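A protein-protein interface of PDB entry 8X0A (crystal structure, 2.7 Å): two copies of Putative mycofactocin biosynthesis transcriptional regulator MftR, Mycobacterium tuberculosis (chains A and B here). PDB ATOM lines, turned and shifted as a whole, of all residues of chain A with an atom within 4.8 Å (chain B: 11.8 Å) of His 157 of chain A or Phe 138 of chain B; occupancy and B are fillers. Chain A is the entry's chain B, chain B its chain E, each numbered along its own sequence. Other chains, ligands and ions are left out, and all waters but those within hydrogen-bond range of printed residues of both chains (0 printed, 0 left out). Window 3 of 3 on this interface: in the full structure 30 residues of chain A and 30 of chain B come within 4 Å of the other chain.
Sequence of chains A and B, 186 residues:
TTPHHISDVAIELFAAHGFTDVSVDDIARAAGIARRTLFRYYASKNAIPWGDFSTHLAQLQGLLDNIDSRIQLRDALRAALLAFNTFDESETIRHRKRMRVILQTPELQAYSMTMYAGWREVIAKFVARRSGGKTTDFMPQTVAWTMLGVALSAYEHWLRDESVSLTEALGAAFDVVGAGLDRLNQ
Hydrophobic or aromatic side chains of chain A within 4 Å of the printed part of chain B: His 157, Ala 169, Ala 172 and Ala 173. Along chain A the printed residues that touch a printed residue of chain B span positions 153 to 173. Among the printed residues, 12 pairs touch across the chains. Among the printed residues, no Asp or Glu carboxylate lies within 4 Å of a Lys or Arg side-chain nitrogen of the other chain.
Of chain B, only Phe 138 (3.6 Å), Gln 141 (3.5 Å), Thr 142 (3.1 Å) and Trp 145 (3.4 Å) come within 4 Å of Ser 153 of chain A. Ala 154 of chain A touches just one residue of chain B: Phe 138 (3.8 Å). No residue of chain B comes within 4 Å of Leu 159 of chain A. Of the printed residues of chain B, Ala 169 of chain A touches Phe 138 (3.1 Å). Ala 173 of chain A touches just these residues of chain B: Phe 138 (3.8 Å) and Thr 142 (3.8 Å). Gly 133 of chain B touches none of the printed residues of chain A. Of the printed residues of chain A, Thr 136 of chain B touches Arg 160. Phe 138 of chain B touches just these residues of chain A: Ser 153 (3.6 Å), Ala 154 (3.8 Å), His 157 (3.6 Å), Ala 169 (3.1 Å), Ala 172 (3.7 Å) and Ala 173 (3.8 Å). Of the printed residues of chain A, Thr 142 of chain B touches Ser 153 (3.1 Å) and Ala 173 (3.8 Å). Of the printed residues of chain A, Trp 145 of chain B touches Ser 153 (3.4 Å) and Glu 156 (3.5 Å).
The backbone carbonyl oxygen (O) of Thr 135 of chain B sits at hydrogen-bond distance from the side-chain amide nitrogen (NE2) of Gln 141 of chain B (2.9 Å). O of Thr 142 of chain B is in hydrogen-bond range of OG1 of Thr 146 of chain B (2.7 Å). The side-chain hydroxyl of Thr 142 of chain B is in hydrogen-bond range of the backbone carbonyl oxygen of Phe 138 of chain B (2.9 Å). The guanidinium group (NH2) of Arg 160 of chain A lies within salt-bridge range of the side-chain carboxylate (OD2) of Asp 161 of chain A (3.9 Å). A ring nitrogen (ND1) of His 157 of chain A sits close to the guanidinium group (NH2) of Arg 160 of chain A, 3.2 Å away.
O of Ser 153 of chain A touches CE1 of Phe 138 of chain B, 3.6 Å away. Ser 153 of chain A touches Gln 141 of chain B (OG to C, 3.5 Å). Ser 153 of chain A touches Trp 145 of chain B (CB to CD1, 3.4 Å). CA of Ala 154 of chain A touches CE1 of Phe 138 of chain B, 3.8 Å away. Phe 138 of chain B touches His 157 of chain A. Thr 136 of chain B touches Arg 160 of chain A (OG1 to CD, 3.1 Å). Ala 169 of chain A touches Phe 138 of chain B (O to CZ, 3.1 Å). CE2 of Phe 138 of chain B touches CB of Ala 172 of chain A (3.7 Å). CZ of Phe 138 of chain B touches CB of Ala 173 of chain A (3.8 Å). Ala 173 of chain A touches Thr 142 of chain B (O to CG2, 3.8 Å).
The side-chain carboxylate (OE1) of Glu 156 of chain A lies within hydrogen-bond range of the indole nitrogen (NE1) of Trp 145 of chain B, 3.5 Å away. The side-chain hydroxyl of Thr 142 of chain B sits at hydrogen-bond distance from the side-chain hydroxyl of Ser 153 of chain A.
No position is printed for both chains. Of the 12 pairs that touch across the chains among the printed residues, none has its exchanged pair printed and touching as well.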
ATOM      1  N   SER A 153       3.445 -22.789  -3.313  1.00  0.00           N
ATOM      2  CA  SER A 153       3.136 -21.458  -3.793  1.00  0.00           C
ATOM      3  C   SER A 153       4.404 -20.712  -4.227  1.00  0.00           C
ATOM      4  O   SER A 153       4.431 -20.102  -5.303  1.00  0.00           O
ATOM      5  CB  SER A 153       2.380 -20.684  -2.734  1.00  0.00           C
ATOM      6  OG  SER A 153       1.891 -19.461  -3.285  1.00  0.00           O
ATOM      7  N   ALA A 154       5.455 -20.774  -3.394  1.00  0.00           N
ATOM      8  CA  ALA A 154       6.732 -20.114  -3.644  1.00  0.00           C
ATOM      9  C   ALA A 154       7.428 -20.712  -4.863  1.00  0.00           C
ATOM     10  O   ALA A 154       7.911 -19.968  -5.721  1.00  0.00           O
ATOM     11  CB  ALA A 154       7.613 -20.207  -2.417  1.00  0.00           C
ATOM     12  N   TYR A 155       7.463 -22.056  -4.912  1.00  0.00           N
ATOM     13  CA  TYR A 155       8.033 -22.790  -6.030  1.00  0.00           C
ATOM     14  C   TYR A 155       7.330 -22.445  -7.335  1.00  0.00           C
ATOM     15  O   TYR A 155       8.026 -22.236  -8.326  1.00  0.00           O
ATOM     16  CB  TYR A 155       8.059 -24.293  -5.753  1.00  0.00           C
ATOM     17  CG  TYR A 155       9.316 -24.725  -5.045  1.00  0.00           C
ATOM     18  CD1 TYR A 155      10.538 -24.646  -5.693  1.00  0.00           C
ATOM     19  CD2 TYR A 155       9.303 -25.223  -3.747  1.00  0.00           C
ATOM     20  CE1 TYR A 155      11.719 -25.023  -5.063  1.00  0.00           C
ATOM     21  CE2 TYR A 155      10.459 -25.675  -3.141  1.00  0.00           C
ATOM     22  CZ  TYR A 155      11.679 -25.557  -3.793  1.00  0.00           C
ATOM     23  OH  TYR A 155      12.858 -25.907  -3.158  1.00  0.00           O
ATOM     24  N   GLU A 156       6.002 -22.330  -7.333  1.00  0.00           N
ATOM     25  CA  GLU A 156       5.297 -22.042  -8.572  1.00  0.00           C
ATOM     26  C   GLU A 156       5.538 -20.603  -9.027  1.00  0.00           C
ATOM     27  O   GLU A 156       5.720 -20.371 -10.216  1.00  0.00           O
ATOM     28  CB  GLU A 156       3.819 -22.340  -8.456  1.00  0.00           C
ATOM     29  CG  GLU A 156       3.538 -23.812  -8.407  1.00  0.00           C
ATOM     30  CD  GLU A 156       2.058 -24.130  -8.552  1.00  0.00           C
ATOM     31  OE1 GLU A 156       1.201 -23.189  -8.331  1.00  0.00           O
ATOM     32  OE2 GLU A 156       1.758 -25.294  -8.916  1.00  0.00           O
ATOM     33  N   HIS A 157       5.555 -19.657  -8.092  1.00  0.00           N
ATOM     34  CA  HIS A 157       5.865 -18.274  -8.411  1.00  0.00           C
ATOM     35  C   HIS A 157       7.280 -18.140  -8.992  1.00  0.00           C
ATOM     36  O   HIS A 157       7.485 -17.424  -9.965  1.00  0.00           O
ATOM     37  CB  HIS A 157       5.700 -17.452  -7.152  1.00  0.00           C
ATOM     38  CG  HIS A 157       5.844 -15.982  -7.348  1.00  0.00           C
ATOM     39  ND1 HIS A 157       5.291 -15.255  -8.374  1.00  0.00           N
ATOM     40  CD2 HIS A 157       6.553 -15.137  -6.566  1.00  0.00           C
ATOM     41  CE1 HIS A 157       5.660 -13.981  -8.211  1.00  0.00           C
ATOM     42  NE2 HIS A 157       6.396 -13.878  -7.060  1.00  0.00           N
ATOM     43  N   TRP A 158       8.224 -18.874  -8.398  1.00  0.00           N
ATOM     44  CA  TRP A 158       9.602 -18.951  -8.846  1.00  0.00           C
ATOM     45  C   TRP A 158       9.758 -19.490 -10.272  1.00  0.00           C
ATOM     46  O   TRP A 158      10.557 -18.937 -11.029  1.00  0.00           O
ATOM     47  CB  TRP A 158      10.357 -19.812  -7.850  1.00  0.00           C
ATOM     48  CG  TRP A 158      11.808 -20.037  -8.115  1.00  0.00           C
ATOM     49  CD1 TRP A 158      12.787 -19.098  -8.154  1.00  0.00           C
ATOM     50  CD2 TRP A 158      12.458 -21.313  -8.249  1.00  0.00           C
ATOM     51  NE1 TRP A 158      14.003 -19.698  -8.316  1.00  0.00           N
ATOM     52  CE2 TRP A 158      13.839 -21.056  -8.409  1.00  0.00           C
ATOM     53  CE3 TRP A 158      12.005 -22.629  -8.296  1.00  0.00           C
ATOM     54  CZ2 TRP A 158      14.775 -22.081  -8.590  1.00  0.00           C
ATOM     55  CZ3 TRP A 158      12.933 -23.638  -8.482  1.00  0.00           C
ATOM     56  CH2 TRP A 158      14.299 -23.372  -8.595  1.00  0.00           C
ATOM     57  N   LEU A 159       9.064 -20.597 -10.594  1.00  0.00           N
ATOM     58  CA  LEU A 159       9.076 -21.191 -11.930  1.00  0.00           C
ATOM     59  C   LEU A 159       8.393 -20.292 -12.971  1.00  0.00           C
ATOM     60  O   LEU A 159       8.829 -20.237 -14.114  1.00  0.00           O
ATOM     61  CB  LEU A 159       8.393 -22.556 -11.870  1.00  0.00           C
ATOM     62  CG  LEU A 159       9.151 -23.654 -11.118  1.00  0.00           C
ATOM     63  CD1 LEU A 159       8.331 -24.944 -11.083  1.00  0.00           C
ATOM     64  CD2 LEU A 159      10.532 -23.885 -11.739  1.00  0.00           C
ATOM     65  N   ARG A 160       7.300 -19.619 -12.594  1.00  0.00           N
ATOM     66  CA  ARG A 160       6.516 -18.806 -13.515  1.00  0.00           C
ATOM     67  C   ARG A 160       7.283 -17.548 -13.926  1.00  0.00           C
ATOM     68  O   ARG A 160       7.107 -17.078 -15.036  1.00  0.00           O
ATOM     69  CB  ARG A 160       5.206 -18.416 -12.827  1.00  0.00           C
ATOM     70  CG  ARG A 160       4.274 -17.515 -13.617  1.00  0.00           C
ATOM     71  CD  ARG A 160       3.145 -16.992 -12.743  1.00  0.00           C
ATOM     72  NE  ARG A 160       3.589 -15.964 -11.799  1.00  0.00           N
ATOM     73  CZ  ARG A 160       3.940 -14.716 -12.122  1.00  0.00           C
ATOM     74  NH1 ARG A 160       3.663 -14.210 -13.314  1.00  0.00           N
ATOM     75  NH2 ARG A 160       4.538 -13.955 -11.222  1.00  0.00           N
ATOM     76  N   ASP A 161       8.115 -17.018 -13.019  1.00  0.00           N
ATOM     77  CA  ASP A 161       8.822 -15.755 -13.156  1.00  0.00           C
ATOM     78  C   ASP A 161      10.271 -16.015 -12.741  1.00  0.00           C
ATOM     79  O   ASP A 161      10.557 -16.196 -11.553  1.00  0.00           O
ATOM     80  CB  ASP A 161       8.162 -14.709 -12.247  1.00  0.00           C
ATOM     81  CG  ASP A 161       8.721 -13.298 -12.300  1.00  0.00           C
ATOM     82  OD1 ASP A 161       9.717 -13.051 -13.011  1.00  0.00           O
ATOM     83  OD2 ASP A 161       8.092 -12.439 -11.661  1.00  0.00           O
ATOM     84  N   VAL A 164      12.516 -13.996  -9.809  1.00  0.00           N
ATOM     85  CA  VAL A 164      12.242 -14.127  -8.388  1.00  0.00           C
ATOM     86  C   VAL A 164      13.384 -14.921  -7.748  1.00  0.00           C
ATOM     87  O   VAL A 164      13.817 -15.936  -8.289  1.00  0.00           O
ATOM     88  CB  VAL A 164      10.907 -14.867  -8.132  1.00  0.00           C
ATOM     89  CG1 VAL A 164      10.577 -14.857  -6.645  1.00  0.00           C
ATOM     90  CG2 VAL A 164       9.712 -14.393  -8.975  1.00  0.00           C
ATOM     91  N   ALA A 169      10.870 -15.652  -2.227  1.00  0.00           N
ATOM     92  CA  ALA A 169       9.542 -16.181  -2.479  1.00  0.00           C
ATOM     93  C   ALA A 169       9.029 -16.980  -1.261  1.00  0.00           C
ATOM     94  O   ALA A 169       7.937 -16.707  -0.733  1.00  0.00           O
ATOM     95  CB  ALA A 169       9.550 -16.971  -3.758  1.00  0.00           C
ATOM     96  N   ALA A 172       8.496 -14.578   1.776  1.00  0.00           N
ATOM     97  CA  ALA A 172       7.287 -13.787   1.585  1.00  0.00           C
ATOM     98  C   ALA A 172       6.030 -14.640   1.844  1.00  0.00           C
ATOM     99  O   ALA A 172       5.127 -14.205   2.577  1.00  0.00           O
ATOM    100  CB  ALA A 172       7.280 -13.179   0.193  1.00  0.00           C
ATOM    101  N   ALA A 173       5.997 -15.849   1.245  1.00  0.00           N
ATOM    102  CA  ALA A 173       4.883 -16.770   1.383  1.00  0.00           C
ATOM    103  C   ALA A 173       4.735 -17.185   2.845  1.00  0.00           C
ATOM    104  O   ALA A 173       3.626 -17.176   3.360  1.00  0.00           O
ATOM    105  CB  ALA A 173       5.054 -17.968   0.466  1.00  0.00           C
ATOM    106  N   LEU B  73     -12.021 -10.440   4.346  1.00  0.00           N
ATOM    107  CA  LEU B  73     -11.516 -11.550   3.542  1.00  0.00           C
ATOM    108  C   LEU B  73     -11.467 -12.842   4.363  1.00  0.00           C
ATOM    109  O   LEU B  73     -11.914 -13.894   3.906  1.00  0.00           O
ATOM    110  CB  LEU B  73     -10.118 -11.191   3.013  1.00  0.00           C
ATOM    111  CG  LEU B  73      -9.406 -12.223   2.142  1.00  0.00           C
ATOM    112  CD1 LEU B  73     -10.151 -12.365   0.829  1.00  0.00           C
ATOM    113  CD2 LEU B  73      -7.941 -11.856   1.918  1.00  0.00           C
ATOM    114  N   ARG B 120      -8.225 -24.160  -5.833  1.00  0.00           N
ATOM    115  CA  ARG B 120      -7.327 -23.025  -5.654  1.00  0.00           C
ATOM    116  C   ARG B 120      -7.582 -21.888  -6.645  1.00  0.00           C
ATOM    117  O   ARG B 120      -7.417 -20.737  -6.255  1.00  0.00           O
ATOM    118  CB  ARG B 120      -5.857 -23.421  -5.764  1.00  0.00           C
ATOM    119  CG  ARG B 120      -5.381 -24.312  -4.620  1.00  0.00           C
ATOM    120  CD  ARG B 120      -3.873 -24.404  -4.571  1.00  0.00           C
ATOM    121  NE  ARG B 120      -3.276 -24.741  -5.853  1.00  0.00           N
ATOM    122  CZ  ARG B 120      -3.097 -25.979  -6.328  1.00  0.00           C
ATOM    123  NH1 ARG B 120      -3.303 -27.050  -5.586  1.00  0.00           N
ATOM    124  NH2 ARG B 120      -2.713 -26.145  -7.574  1.00  0.00           N
ATOM    125  N   GLU B 121      -7.975 -22.181  -7.888  1.00  0.00           N
ATOM    126  CA  GLU B 121      -8.311 -21.127  -8.841  1.00  0.00           C
ATOM    127  C   GLU B 121      -9.517 -20.314  -8.350  1.00  0.00           C
ATOM    128  O   GLU B 121      -9.515 -19.093  -8.488  1.00  0.00           O
ATOM    129  CB  GLU B 121      -8.533 -21.651 -10.266  1.00  0.00           C
ATOM    130  CG  GLU B 121      -8.541 -20.521 -11.305  1.00  0.00           C
ATOM    131  CD  GLU B 121      -8.766 -20.835 -12.772  1.00  0.00           C
ATOM    132  OE1 GLU B 121      -8.791 -22.008 -13.141  1.00  0.00           O
ATOM    133  OE2 GLU B 121      -8.937 -19.869 -13.550  1.00  0.00           O
ATOM    134  N   ILE B 123     -10.466 -19.823  -5.170  1.00  0.00           N
ATOM    135  CA  ILE B 123     -10.027 -19.046  -4.014  1.00  0.00           C
ATOM    136  C   ILE B 123      -9.219 -17.825  -4.465  1.00  0.00           C
ATOM    137  O   ILE B 123      -9.421 -16.704  -3.961  1.00  0.00           O
ATOM    138  CB  ILE B 123      -9.209 -19.902  -3.016  1.00  0.00           C
ATOM    139  CG1 ILE B 123      -9.959 -21.112  -2.443  1.00  0.00           C
ATOM    140  CG2 ILE B 123      -8.654 -19.028  -1.894  1.00  0.00           C
ATOM    141  CD1 ILE B 123     -11.285 -20.795  -1.851  1.00  0.00           C
ATOM    142  N   ALA B 124      -8.249 -18.065  -5.370  1.00  0.00           N
ATOM    143  CA  ALA B 124      -7.375 -17.013  -5.849  1.00  0.00           C
ATOM    144  C   ALA B 124      -8.143 -15.940  -6.631  1.00  0.00           C
ATOM    145  O   ALA B 124      -7.846 -14.750  -6.485  1.00  0.00           O
ATOM    146  CB  ALA B 124      -6.298 -17.666  -6.650  1.00  0.00           C
ATOM    147  N   LYS B 125      -9.131 -16.363  -7.460  1.00  0.00           N
ATOM    148  CA  LYS B 125     -10.012 -15.443  -8.180  1.00  0.00           C
ATOM    149  C   LYS B 125     -10.722 -14.507  -7.208  1.00  0.00           C
ATOM    150  O   LYS B 125     -10.805 -13.312  -7.470  1.00  0.00           O
ATOM    151  CB  LYS B 125     -11.080 -16.170  -9.007  1.00  0.00           C
ATOM    152  CG  LYS B 125     -10.799 -16.399 -10.483  1.00  0.00           C
ATOM    153  CD  LYS B 125     -11.938 -17.228 -11.118  1.00  0.00           C
ATOM    154  CE  LYS B 125     -11.648 -17.851 -12.474  1.00  0.00           C
ATOM    155  NZ  LYS B 125     -11.500 -16.821 -13.530  1.00  0.00           N
ATOM    156  N   VAL B 127      -9.803 -13.577  -4.140  1.00  0.00           N
ATOM    157  CA  VAL B 127      -8.840 -12.652  -3.539  1.00  0.00           C
ATOM    158  C   VAL B 127      -8.490 -11.559  -4.561  1.00  0.00           C
ATOM    159  O   VAL B 127      -8.417 -10.391  -4.195  1.00  0.00           O
ATOM    160  CB  VAL B 127      -7.578 -13.397  -3.043  1.00  0.00           C
ATOM    161  CG1 VAL B 127      -6.478 -12.441  -2.586  1.00  0.00           C
ATOM    162  CG2 VAL B 127      -7.878 -14.448  -1.980  1.00  0.00           C
ATOM    163  N   ALA B 128      -8.245 -11.954  -5.831  1.00  0.00           N
ATOM    164  CA  ALA B 128      -7.932 -11.012  -6.905  1.00  0.00           C
ATOM    165  C   ALA B 128      -9.111 -10.033  -7.057  1.00  0.00           C
ATOM    166  O   ALA B 128      -8.880  -8.825  -7.067  1.00  0.00           O
ATOM    167  CB  ALA B 128      -7.514 -11.738  -8.192  1.00  0.00           C
ATOM    168  N   SER B 131      -8.812  -7.532  -4.189  1.00  0.00           N
ATOM    169  CA  SER B 131      -7.568  -6.780  -4.150  1.00  0.00           C
ATOM    170  C   SER B 131      -7.330  -6.247  -5.573  1.00  0.00           C
ATOM    171  O   SER B 131      -8.271  -6.145  -6.349  1.00  0.00           O
ATOM    172  CB  SER B 131      -6.476  -7.711  -3.680  1.00  0.00           C
ATOM    173  OG  SER B 131      -6.903  -8.492  -2.573  1.00  0.00           O
ATOM    174  N   GLY B 132      -6.088  -5.936  -5.955  1.00  0.00           N
ATOM    175  CA  GLY B 132      -5.727  -5.817  -7.355  1.00  0.00           C
ATOM    176  C   GLY B 132      -5.898  -7.112  -8.147  1.00  0.00           C
ATOM    177  O   GLY B 132      -5.841  -8.220  -7.592  1.00  0.00           O
ATOM    178  N   GLY B 133      -6.001  -6.961  -9.477  1.00  0.00           N
ATOM    179  CA  GLY B 133      -6.230  -8.085 -10.381  1.00  0.00           C
ATOM    180  C   GLY B 133      -5.027  -9.027 -10.511  1.00  0.00           C
ATOM    181  O   GLY B 133      -3.924  -8.702 -10.109  1.00  0.00           O
ATOM    182  N   LYS B 134      -5.286 -10.229 -11.020  1.00  0.00           N
ATOM    183  CA  LYS B 134      -4.342 -11.234 -11.512  1.00  0.00           C
ATOM    184  C   LYS B 134      -4.231 -12.386 -10.498  1.00  0.00           C
ATOM    185  O   LYS B 134      -3.494 -12.328  -9.503  1.00  0.00           O
ATOM    186  CB  LYS B 134      -3.041 -10.706 -12.143  1.00  0.00           C
ATOM    187  CG  LYS B 134      -2.607 -11.425 -13.432  1.00  0.00           C
ATOM    188  CD  LYS B 134      -1.909 -10.558 -14.468  1.00  0.00           C
ATOM    189  CE  LYS B 134      -1.959 -11.151 -15.864  1.00  0.00           C
ATOM    190  NZ  LYS B 134      -1.355 -12.511 -15.924  1.00  0.00           N
ATOM    191  N   THR B 135      -5.025 -13.441 -10.812  1.00  0.00           N
ATOM    192  CA  THR B 135      -5.153 -14.722 -10.121  1.00  0.00           C
ATOM    193  C   THR B 135      -3.799 -15.349  -9.793  1.00  0.00           C
ATOM    194  O   THR B 135      -3.669 -15.991  -8.754  1.00  0.00           O
ATOM    195  CB  THR B 135      -5.997 -15.670 -11.001  1.00  0.00           C
ATOM    196  OG1 THR B 135      -7.349 -15.233 -10.883  1.00  0.00           O
ATOM    197  CG2 THR B 135      -5.952 -17.143 -10.649  1.00  0.00           C
ATOM    198  N   THR B 136      -2.826 -15.177 -10.707  1.00  0.00           N
ATOM    199  CA  THR B 136      -1.491 -15.736 -10.609  1.00  0.00           C
ATOM    200  C   THR B 136      -0.531 -14.921  -9.730  1.00  0.00           C
ATOM    201  O   THR B 136       0.599 -15.354  -9.533  1.00  0.00           O
ATOM    202  CB  THR B 136      -0.922 -15.850 -12.029  1.00  0.00           C
ATOM    203  OG1 THR B 136       0.135 -16.789 -11.884  1.00  0.00           O
ATOM    204  CG2 THR B 136      -0.467 -14.519 -12.595  1.00  0.00           C
ATOM    205  N   ASP B 137      -0.945 -13.758  -9.189  1.00  0.00           N
ATOM    206  CA  ASP B 137      -0.089 -12.976  -8.313  1.00  0.00           C
ATOM    207  C   ASP B 137       0.221 -13.768  -7.050  1.00  0.00           C
ATOM    208  O   ASP B 137      -0.479 -14.726  -6.738  1.00  0.00           O
ATOM    209  CB  ASP B 137      -0.716 -11.617  -8.001  1.00  0.00           C
ATOM    210  CG  ASP B 137      -0.791 -10.684  -9.207  1.00  0.00           C
ATOM    211  OD1 ASP B 137      -0.056 -10.948 -10.199  1.00  0.00           O
ATOM    212  OD2 ASP B 137      -1.585  -9.713  -9.169  1.00  0.00           O
ATOM    213  N   PHE B 138       1.249 -13.339  -6.324  1.00  0.00           N
ATOM    214  CA  PHE B 138       1.777 -14.132  -5.224  1.00  0.00           C
ATOM    215  C   PHE B 138       0.760 -14.337  -4.092  1.00  0.00           C
ATOM    216  O   PHE B 138       0.557 -15.462  -3.643  1.00  0.00           O
ATOM    217  CB  PHE B 138       3.077 -13.543  -4.662  1.00  0.00           C
ATOM    218  CG  PHE B 138       3.996 -14.569  -4.047  1.00  0.00           C
ATOM    219  CD1 PHE B 138       3.832 -15.952  -4.237  1.00  0.00           C
ATOM    220  CD2 PHE B 138       5.079 -14.142  -3.291  1.00  0.00           C
ATOM    221  CE1 PHE B 138       4.719 -16.859  -3.680  1.00  0.00           C
ATOM    222  CE2 PHE B 138       5.973 -15.060  -2.748  1.00  0.00           C
ATOM    223  CZ  PHE B 138       5.785 -16.412  -2.935  1.00  0.00           C
ATOM    224  N   MET B 139       0.142 -13.240  -3.636  1.00  0.00           N
ATOM    225  CA  MET B 139      -0.753 -13.214  -2.490  1.00  0.00           C
ATOM    226  C   MET B 139      -2.021 -14.060  -2.747  1.00  0.00           C
ATOM    227  O   MET B 139      -2.295 -14.961  -1.973  1.00  0.00           O
ATOM    228  CB  MET B 139      -1.043 -11.739  -2.145  1.00  0.00           C
ATOM    229  CG  MET B 139      -2.270 -11.419  -1.304  1.00  0.00           C
ATOM    230  SD  MET B 139      -2.042 -12.153   0.274  1.00  0.00           S
ATOM    231  CE  MET B 139      -3.586 -11.632   1.033  1.00  0.00           C
ATOM    232  N   PRO B 140      -2.847 -13.862  -3.805  1.00  0.00           N
ATOM    233  CA  PRO B 140      -3.941 -14.794  -4.103  1.00  0.00           C
ATOM    234  C   PRO B 140      -3.594 -16.285  -4.127  1.00  0.00           C
ATOM    235  O   PRO B 140      -4.352 -17.142  -3.660  1.00  0.00           O
ATOM    236  CB  PRO B 140      -4.404 -14.389  -5.518  1.00  0.00           C
ATOM    237  CG  PRO B 140      -3.847 -13.012  -5.812  1.00  0.00           C
ATOM    238  CD  PRO B 140      -2.789 -12.754  -4.769  1.00  0.00           C
ATOM    239  N   GLN B 141      -2.393 -16.575  -4.622  1.00  0.00           N
ATOM    240  CA  GLN B 141      -1.878 -17.926  -4.857  1.00  0.00           C
ATOM    241  C   GLN B 141      -1.503 -18.544  -3.513  1.00  0.00           C
ATOM    242  O   GLN B 141      -1.857 -19.698  -3.257  1.00  0.00           O
ATOM    243  CB  GLN B 141      -0.676 -17.899  -5.833  1.00  0.00           C
ATOM    244  CG  GLN B 141      -1.006 -17.862  -7.326  1.00  0.00           C
ATOM    245  CD  GLN B 141      -1.817 -19.054  -7.800  1.00  0.00           C
ATOM    246  OE1 GLN B 141      -1.511 -20.198  -7.460  1.00  0.00           O
ATOM    247  NE2 GLN B 141      -2.909 -18.797  -8.521  1.00  0.00           N
ATOM    248  N   THR B 142      -0.789 -17.758  -2.681  1.00  0.00           N
ATOM    249  CA  THR B 142      -0.418 -18.144  -1.325  1.00  0.00           C
ATOM    250  C   THR B 142      -1.670 -18.383  -0.472  1.00  0.00           C
ATOM    251  O   THR B 142      -1.704 -19.338   0.292  1.00  0.00           O
ATOM    252  CB  THR B 142       0.540 -17.131  -0.666  1.00  0.00           C
ATOM    253  OG1 THR B 142       1.701 -16.948  -1.496  1.00  0.00           O
ATOM    254  CG2 THR B 142       0.958 -17.557   0.728  1.00  0.00           C
ATOM    255  N   VAL B 143      -2.680 -17.523  -0.604  1.00  0.00           N
ATOM    256  CA  VAL B 143      -3.912 -17.679   0.140  1.00  0.00           C
ATOM    257  C   VAL B 143      -4.629 -18.967  -0.305  1.00  0.00           C
ATOM    258  O   VAL B 143      -5.147 -19.695   0.543  1.00  0.00           O
ATOM    259  CB  VAL B 143      -4.823 -16.431   0.049  1.00  0.00           C
ATOM    260  CG1 VAL B 143      -6.164 -16.667   0.738  1.00  0.00           C
ATOM    261  CG2 VAL B 143      -4.175 -15.177   0.623  1.00  0.00           C
ATOM    262  N   ALA B 144      -4.638 -19.265  -1.617  1.00  0.00           N
ATOM    263  CA  ALA B 144      -5.296 -20.466  -2.130  1.00  0.00           C
ATOM    264  C   ALA B 144      -4.635 -21.746  -1.635  1.00  0.00           C
ATOM    265  O   ALA B 144      -5.324 -22.673  -1.264  1.00  0.00           O
ATOM    266  CB  ALA B 144      -5.306 -20.429  -3.634  1.00  0.00           C
ATOM    267  N   TRP B 145      -3.301 -21.787  -1.674  1.00  0.00           N
ATOM    268  CA  TRP B 145      -2.493 -22.909  -1.199  1.00  0.00           C
ATOM    269  C   TRP B 145      -2.629 -23.101   0.311  1.00  0.00           C
ATOM    270  O   TRP B 145      -2.629 -24.238   0.798  1.00  0.00           O
ATOM    271  CB  TRP B 145      -1.001 -22.708  -1.537  1.00  0.00           C
ATOM    272  CG  TRP B 145      -0.611 -23.179  -2.909  1.00  0.00           C
ATOM    273  CD1 TRP B 145      -0.261 -22.396  -3.971  1.00  0.00           C
ATOM    274  CD2 TRP B 145      -0.463 -24.539  -3.359  1.00  0.00           C
ATOM    275  NE1 TRP B 145       0.085 -23.167  -5.036  1.00  0.00           N
ATOM    276  CE2 TRP B 145      -0.027 -24.484  -4.704  1.00  0.00           C
ATOM    277  CE3 TRP B 145      -0.677 -25.799  -2.774  1.00  0.00           C
ATOM    278  CZ2 TRP B 145       0.198 -25.628  -5.469  1.00  0.00           C
ATOM    279  CZ3 TRP B 145      -0.433 -26.936  -3.515  1.00  0.00           C
ATOM    280  CH2 TRP B 145       0.002 -26.846  -4.846  1.00  0.00           C
ATOM    281  N   THR B 146      -2.614 -21.984   1.049  1.00  0.00           N
ATOM    282  CA  THR B 146      -2.808 -21.992   2.488  1.00  0.00           C
ATOM    283  C   THR B 146      -4.155 -22.630   2.836  1.00  0.00           C
ATOM    284  O   THR B 146      -4.225 -23.512   3.666  1.00  0.00           O
ATOM    285  CB  THR B 146      -2.695 -20.569   3.033  1.00  0.00           C
ATOM    286  OG1 THR B 146      -1.332 -20.149   2.852  1.00  0.00           O
ATOM    287  CG2 THR B 146      -3.118 -20.460   4.486  1.00  0.00           C
ATOM    288  N   MET B 147      -5.206 -22.165   2.167  1.00  0.00           N
ATOM    289  CA  MET B 147      -6.553 -22.683   2.287  1.00  0.00           C
ATOM    290  C   MET B 147      -6.610 -24.179   1.952  1.00  0.00           C
ATOM    291  O   MET B 147      -7.372 -24.940   2.573  1.00  0.00           O
ATOM    292  CB  MET B 147      -7.492 -21.936   1.327  1.00  0.00           C
ATOM    293  CG  MET B 147      -8.006 -20.545   1.672  1.00  0.00           C
ATOM    294  SD  MET B 147      -8.971 -20.395   3.165  1.00  0.00           S
ATOM    295  CE  MET B 147      -7.576 -20.383   4.291  1.00  0.00           C
